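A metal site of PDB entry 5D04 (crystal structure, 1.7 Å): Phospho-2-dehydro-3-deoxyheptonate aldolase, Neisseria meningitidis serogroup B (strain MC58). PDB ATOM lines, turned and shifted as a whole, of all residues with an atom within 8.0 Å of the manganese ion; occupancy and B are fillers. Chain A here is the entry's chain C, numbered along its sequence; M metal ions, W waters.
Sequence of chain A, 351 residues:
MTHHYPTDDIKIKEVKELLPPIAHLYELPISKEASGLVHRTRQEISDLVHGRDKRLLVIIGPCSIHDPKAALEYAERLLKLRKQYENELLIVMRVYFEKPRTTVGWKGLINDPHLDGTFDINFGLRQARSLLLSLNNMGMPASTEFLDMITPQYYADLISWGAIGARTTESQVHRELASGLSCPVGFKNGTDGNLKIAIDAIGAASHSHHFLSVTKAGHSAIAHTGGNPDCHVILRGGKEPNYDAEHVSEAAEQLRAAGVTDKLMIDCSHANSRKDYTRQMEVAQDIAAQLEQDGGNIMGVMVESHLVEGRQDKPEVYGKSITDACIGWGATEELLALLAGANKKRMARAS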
ATOM      1  N   GLY A  61      14.089  26.079  32.368  1.00  0.00           N
ATOM      2  CA  GLY A  61      13.211  25.107  32.935  1.00  0.00           C
ATOM      3  C   GLY A  61      13.172  23.845  32.137  1.00  0.00           C
ATOM      4  O   GLY A  61      14.028  23.597  31.296  1.00  0.00           O
ATOM      5  N   PRO A  62      12.212  22.990  32.438  1.00  0.00           N
ATOM      6  CA  PRO A  62      12.231  21.707  31.767  1.00  0.00           C
ATOM      7  C   PRO A  62      12.117  21.790  30.250  1.00  0.00           C
ATOM      8  O   PRO A  62      11.497  22.716  29.710  1.00  0.00           O
ATOM      9  CB  PRO A  62      10.995  21.035  32.337  1.00  0.00           C
ATOM     10  CG  PRO A  62      10.879  21.607  33.747  1.00  0.00           C
ATOM     11  CD  PRO A  62      11.249  23.034  33.559  1.00  0.00           C
ATOM     12  N   CYS A  63      12.649  20.805  29.561  1.00  0.00           N
ATOM     13  CA  CYS A  63      12.422  20.676  28.113  1.00  0.00           C
ATOM     14  C   CYS A  63      10.930  20.700  27.813  1.00  0.00           C
ATOM     15  O   CYS A  63      10.485  21.471  26.964  1.00  0.00           O
ATOM     16  CB  CYS A  63      13.032  19.399  27.556  1.00  0.00           C
ATOM     17  SG  CYS A  63      12.667  19.107  25.783  1.00  0.00           S
ATOM     18  N   SER A  64      10.192  19.837  28.509  1.00  0.00           N
ATOM     19  CA  SER A  64       8.745  19.746  28.444  1.00  0.00           C
ATOM     20  C   SER A  64       8.187  19.499  29.833  1.00  0.00           C
ATOM     21  O   SER A  64       8.851  18.881  30.657  1.00  0.00           O
ATOM     22  CB  SER A  64       8.309  18.615  27.525  1.00  0.00           C
ATOM     23  OG  SER A  64       8.642  17.363  28.035  1.00  0.00           O
ATOM     24  N   ARG A  94      10.597  28.180  31.695  1.00  0.00           N
ATOM     25  CA  ARG A  94      10.194  27.402  30.535  1.00  0.00           C
ATOM     26  C   ARG A  94       9.024  26.576  30.880  1.00  0.00           C
ATOM     27  O   ARG A  94       9.106  25.743  31.784  1.00  0.00           O
ATOM     28  CB  ARG A  94      11.303  26.439  30.102  1.00  0.00           C
ATOM     29  CG  ARG A  94      12.309  26.963  29.120  1.00  0.00           C
ATOM     30  CD  ARG A  94      13.224  25.805  28.657  1.00  0.00           C
ATOM     31  NE  ARG A  94      12.566  24.717  27.901  1.00  0.00           N
ATOM     32  CZ  ARG A  94      12.566  24.618  26.559  1.00  0.00           C
ATOM     33  NH1 ARG A  94      13.219  25.511  25.827  1.00  0.00           N
ATOM     34  NH2 ARG A  94      11.996  23.606  25.954  1.00  0.00           N
ATOM     35  N   TYR A  96       6.949  24.665  28.381  1.00  0.00           N
ATOM     36  CA  TYR A  96       6.678  24.125  27.065  1.00  0.00           C
ATOM     37  C   TYR A  96       5.952  22.839  27.279  1.00  0.00           C
ATOM     38  O   TYR A  96       6.396  21.996  28.078  1.00  0.00           O
ATOM     39  CB  TYR A  96       7.962  23.832  26.294  1.00  0.00           C
ATOM     40  CG  TYR A  96       8.742  25.020  25.802  1.00  0.00           C
ATOM     41  CD1 TYR A  96       9.018  26.117  26.616  1.00  0.00           C
ATOM     42  CD2 TYR A  96       9.247  25.018  24.504  1.00  0.00           C
ATOM     43  CE1 TYR A  96       9.750  27.202  26.136  1.00  0.00           C
ATOM     44  CE2 TYR A  96       9.986  26.073  24.039  1.00  0.00           C
ATOM     45  CZ  TYR A  96      10.220  27.163  24.834  1.00  0.00           C
ATOM     46  OH  TYR A  96      11.018  28.188  24.338  1.00  0.00           O
ATOM     47  N   GLU A  98       5.221  20.502  24.898  1.00  0.00           N
ATOM     48  CA  GLU A  98       5.489  19.477  23.893  1.00  0.00           C
ATOM     49  C   GLU A  98       6.893  19.733  23.320  1.00  0.00           C
ATOM     50  O   GLU A  98       7.323  20.870  23.247  1.00  0.00           O
ATOM     51  CB  GLU A  98       4.430  19.599  22.767  1.00  0.00           C
ATOM     52  CG  GLU A  98       4.685  18.662  21.630  1.00  0.00           C
ATOM     53  CD  GLU A  98       3.549  18.626  20.612  1.00  0.00           C
ATOM     54  OE1 GLU A  98       3.680  17.776  19.709  1.00  0.00           O
ATOM     55  OE2 GLU A  98       2.587  19.401  20.709  1.00  0.00           O
ATOM     56  N   LYS A  99       7.582  18.668  22.964  1.00  0.00           N
ATOM     57  CA  LYS A  99       8.793  18.766  22.135  1.00  0.00           C
ATOM     58  C   LYS A  99       8.403  18.301  20.705  1.00  0.00           C
ATOM     59  O   LYS A  99       8.076  17.149  20.537  1.00  0.00           O
ATOM     60  CB  LYS A  99       9.854  17.834  22.725  1.00  0.00           C
ATOM     61  CG  LYS A  99      10.920  17.387  21.768  1.00  0.00           C
ATOM     62  CD  LYS A  99      12.221  18.101  21.938  1.00  0.00           C
ATOM     63  CE  LYS A  99      13.281  17.429  21.061  1.00  0.00           C
ATOM     64  NZ  LYS A  99      14.305  18.440  20.739  1.00  0.00           N
ATOM     65  N   PRO A 100       8.483  19.190  19.687  1.00  0.00           N
ATOM     66  CA  PRO A 100       8.217  18.707  18.324  1.00  0.00           C
ATOM     67  C   PRO A 100       9.294  17.733  17.909  1.00  0.00           C
ATOM     68  O   PRO A 100      10.461  17.887  18.304  1.00  0.00           O
ATOM     69  CB  PRO A 100       8.241  19.959  17.460  1.00  0.00           C
ATOM     70  CG  PRO A 100       8.933  21.012  18.276  1.00  0.00           C
ATOM     71  CD  PRO A 100       8.866  20.611  19.725  1.00  0.00           C
ATOM     72  N   ARG A 167      11.948  24.669  13.525  1.00  0.00           N
ATOM     73  CA  ARG A 167      11.199  23.981  12.466  1.00  0.00           C
ATOM     74  C   ARG A 167      10.029  24.798  11.904  1.00  0.00           C
ATOM     75  O   ARG A 167       9.417  24.371  10.899  1.00  0.00           O
ATOM     76  CB  ARG A 167      10.648  22.662  12.981  1.00  0.00           C
ATOM     77  CG  ARG A 167      11.725  21.650  13.368  1.00  0.00           C
ATOM     78  CD  ARG A 167      11.123  20.543  14.228  1.00  0.00           C
ATOM     79  NE  ARG A 167      12.169  19.659  14.775  1.00  0.00           N
ATOM     80  CZ  ARG A 167      12.930  19.915  15.874  1.00  0.00           C
ATOM     81  NH1 ARG A 167      13.841  19.030  16.230  1.00  0.00           N
ATOM     82  NH2 ARG A 167      12.817  21.046  16.596  1.00  0.00           N
ATOM     83  N   LYS A 188      13.934  31.083  16.436  1.00  0.00           N
ATOM     84  CA  LYS A 188      15.159  30.293  16.356  1.00  0.00           C
ATOM     85  C   LYS A 188      15.691  30.185  14.944  1.00  0.00           C
ATOM     86  O   LYS A 188      14.917  30.119  13.975  1.00  0.00           O
ATOM     87  CB  LYS A 188      14.934  28.894  16.915  1.00  0.00           C
ATOM     88  CG  LYS A 188      15.121  28.865  18.418  1.00  0.00           C
ATOM     89  CD  LYS A 188      14.823  27.561  19.104  1.00  0.00           C
ATOM     90  CE  LYS A 188      15.487  27.575  20.454  1.00  0.00           C
ATOM     91  NZ  LYS A 188      15.466  26.254  21.131  1.00  0.00           N
ATOM     92  N   ASP A 267      20.638  29.876  22.950  1.00  0.00           N
ATOM     93  CA  ASP A 267      20.195  28.625  23.579  1.00  0.00           C
ATOM     94  C   ASP A 267      21.465  27.829  23.947  1.00  0.00           C
ATOM     95  O   ASP A 267      22.318  27.582  23.096  1.00  0.00           O
ATOM     96  CB  ASP A 267      19.327  27.852  22.596  1.00  0.00           C
ATOM     97  CG  ASP A 267      18.685  26.597  23.198  1.00  0.00           C
ATOM     98  OD1 ASP A 267      18.911  26.248  24.369  1.00  0.00           O
ATOM     99  OD2 ASP A 267      17.899  25.978  22.419  1.00  0.00           O
ATOM    100  N   SER A 269      21.297  24.771  25.058  1.00  0.00           N
ATOM    101  CA  SER A 269      20.937  23.371  24.922  1.00  0.00           C
ATOM    102  C   SER A 269      20.768  23.041  23.445  1.00  0.00           C
ATOM    103  O   SER A 269      21.310  23.747  22.587  1.00  0.00           O
ATOM    104  CB  SER A 269      19.672  23.104  25.726  1.00  0.00           C
ATOM    105  OG  SER A 269      19.505  21.705  25.965  1.00  0.00           O
ATOM    106  N   HIS A 270      20.049  21.962  23.157  1.00  0.00           N
ATOM    107  CA  HIS A 270      19.786  21.501  21.786  1.00  0.00           C
ATOM    108  C   HIS A 270      21.111  21.439  21.009  1.00  0.00           C
ATOM    109  O   HIS A 270      22.052  20.843  21.516  1.00  0.00           O
ATOM    110  CB  HIS A 270      18.696  22.345  21.152  1.00  0.00           C
ATOM    111  CG  HIS A 270      17.446  22.347  21.973  1.00  0.00           C
ATOM    112  ND1 HIS A 270      17.026  23.449  22.665  1.00  0.00           N
ATOM    113  CD2 HIS A 270      16.566  21.356  22.287  1.00  0.00           C
ATOM    114  CE1 HIS A 270      15.929  23.167  23.355  1.00  0.00           C
ATOM    115  NE2 HIS A 270      15.631  21.901  23.134  1.00  0.00           N
ATOM    116  N   MET A 302      18.911  30.593  26.978  1.00  0.00           N
ATOM    117  CA  MET A 302      17.920  29.529  27.222  1.00  0.00           C
ATOM    118  C   MET A 302      18.643  28.318  27.792  1.00  0.00           C
ATOM    119  O   MET A 302      19.752  27.997  27.361  1.00  0.00           O
ATOM    120  CB  MET A 302      17.236  29.204  25.904  1.00  0.00           C
ATOM    121  CG  MET A 302      16.212  28.095  25.994  1.00  0.00           C
ATOM    122  SD  MET A 302      15.264  27.918  24.455  1.00  0.00           S
ATOM    123  CE  MET A 302      15.596  29.468  23.632  1.00  0.00           C
ATOM    124  N   GLU A 304      17.872  24.248  29.574  1.00  0.00           N
ATOM    125  CA  GLU A 304      16.965  23.158  29.874  1.00  0.00           C
ATOM    126  C   GLU A 304      17.451  22.521  31.188  1.00  0.00           C
ATOM    127  O   GLU A 304      18.550  21.957  31.266  1.00  0.00           O
ATOM    128  CB  GLU A 304      16.928  22.132  28.747  1.00  0.00           C
ATOM    129  CG  GLU A 304      16.275  22.725  27.508  1.00  0.00           C
ATOM    130  CD  GLU A 304      15.970  21.712  26.429  1.00  0.00           C
ATOM    131  OE1 GLU A 304      16.905  21.052  25.924  1.00  0.00           O
ATOM    132  OE2 GLU A 304      14.788  21.607  26.097  1.00  0.00           O
ATOM    133  N   SER A 321      13.152  14.712  33.157  1.00  0.00           N
ATOM    134  CA  SER A 321      12.624  14.874  31.809  1.00  0.00           C
ATOM    135  C   SER A 321      12.318  13.554  31.123  1.00  0.00           C
ATOM    136  O   SER A 321      13.128  12.628  31.210  1.00  0.00           O
ATOM    137  CB  SER A 321      13.649  15.608  30.920  1.00  0.00           C
ATOM    138  OG  SER A 321      13.086  15.819  29.620  1.00  0.00           O
ATOM    139  N   THR A 323      11.623  14.071  27.740  1.00  0.00           N
ATOM    140  CA  THR A 323      12.014  14.539  26.415  1.00  0.00           C
ATOM    141  C   THR A 323      13.521  14.810  26.422  1.00  0.00           C
ATOM    142  O   THR A 323      14.247  13.899  26.765  1.00  0.00           O
ATOM    143  CB  THR A 323      11.124  15.706  25.919  1.00  0.00           C
ATOM    144  OG1 THR A 323      11.081  16.757  26.894  1.00  0.00           O
ATOM    145  CG2 THR A 323       9.676  15.187  25.636  1.00  0.00           C
ATOM    146  N   ASP A 324      14.019  16.002  26.105  1.00  0.00           N
ATOM    147  CA  ASP A 324      15.462  16.204  26.080  1.00  0.00           C
ATOM    148  C   ASP A 324      16.032  16.162  27.503  1.00  0.00           C
ATOM    149  O   ASP A 324      15.351  16.566  28.459  1.00  0.00           O
ATOM    150  CB  ASP A 324      15.863  17.546  25.453  1.00  0.00           C
ATOM    151  CG  ASP A 324      15.457  17.678  23.983  1.00  0.00           C
ATOM    152  OD1 ASP A 324      15.460  16.657  23.265  1.00  0.00           O
ATOM    153  OD2 ASP A 324      15.170  18.817  23.530  1.00  0.00           O
ATOM    154  N   ALA A 325      17.262  15.689  27.627  1.00  0.00           N
ATOM    155  CA  ALA A 325      17.911  15.667  28.914  1.00  0.00           C
ATOM    156  C   ALA A 325      18.187  17.082  29.411  1.00  0.00           C
ATOM    157  O   ALA A 325      18.522  17.979  28.624  1.00  0.00           O
ATOM    158  CB  ALA A 325      19.201  14.839  28.874  1.00  0.00           C
ATOM    159  N   CYS A 326      18.026  17.265  30.725  1.00  0.00           N
ATOM    160  CA  CYS A 326      18.176  18.567  31.349  1.00  0.00           C
ATOM    161  C   CYS A 326      19.266  18.475  32.407  1.00  0.00           C
ATOM    162  O   CYS A 326      19.565  17.386  32.914  1.00  0.00           O
ATOM    163  CB  CYS A 326      16.881  18.968  32.052  1.00  0.00           C
ATOM    164  SG  CYS A 326      15.501  19.223  30.919  1.00  0.00           S
HETATM  165 MN    MN M   1      14.278  20.465  24.412  1.00  0.00          MN
HETATM  166  O   HOH W   1      12.606  21.216  23.170  1.00  0.00           O
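CD of Lys 99 touches the manganese ion (3.99 Å).
The nearest printed residue that does not touch the manganese ion is Arg 94 (4.2 Å).
N of Cys 63 is in hydrogen-bond range of SG of Cys 326, 3.5 Å away.
The side-chain hydroxyl of Ser 321 sits at hydrogen-bond distance from the backbone carbonyl oxygen of Asp 324, at 2.7 Å.
OG1 of Thr 323 sits close to SG of Cys 63 (3.0 Å).
The side-chain carboxylate (OE1) of Glu 304 is in hydrogen-bond range of the side-chain hydroxyl (OG) of Ser 269 (2.7 Å).
The guanidinium group (NH2) of Arg 94 lies close to the side-chain carboxylate (OE2) of Glu 304, at 3.4 Å.
The backbone carbonyl oxygen (O) of Asp 324 is in hydrogen-bond range of the side-chain sulfur (SG) of Cys 326, 3.6 Å away.
A ring nitrogen (ND1) of His 270 lies within hydrogen-bond range of the side-chain carboxylate (OD2) of Asp 267 (2.7 Å).
O of Cys 63 is in hydrogen-bond range of NH2 of Arg 94 (2.8 Å).
The manganese ion is bound by OD2 of Asp 324 (2.1 Å), OE2 of Glu 304 (2.1 Å), water W1 (2.2 Å), NE2 of His 270 (2.4 Å) and SG of Cys 63 (2.5 Å).
The manganese ion has five donor atoms within binding distance.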
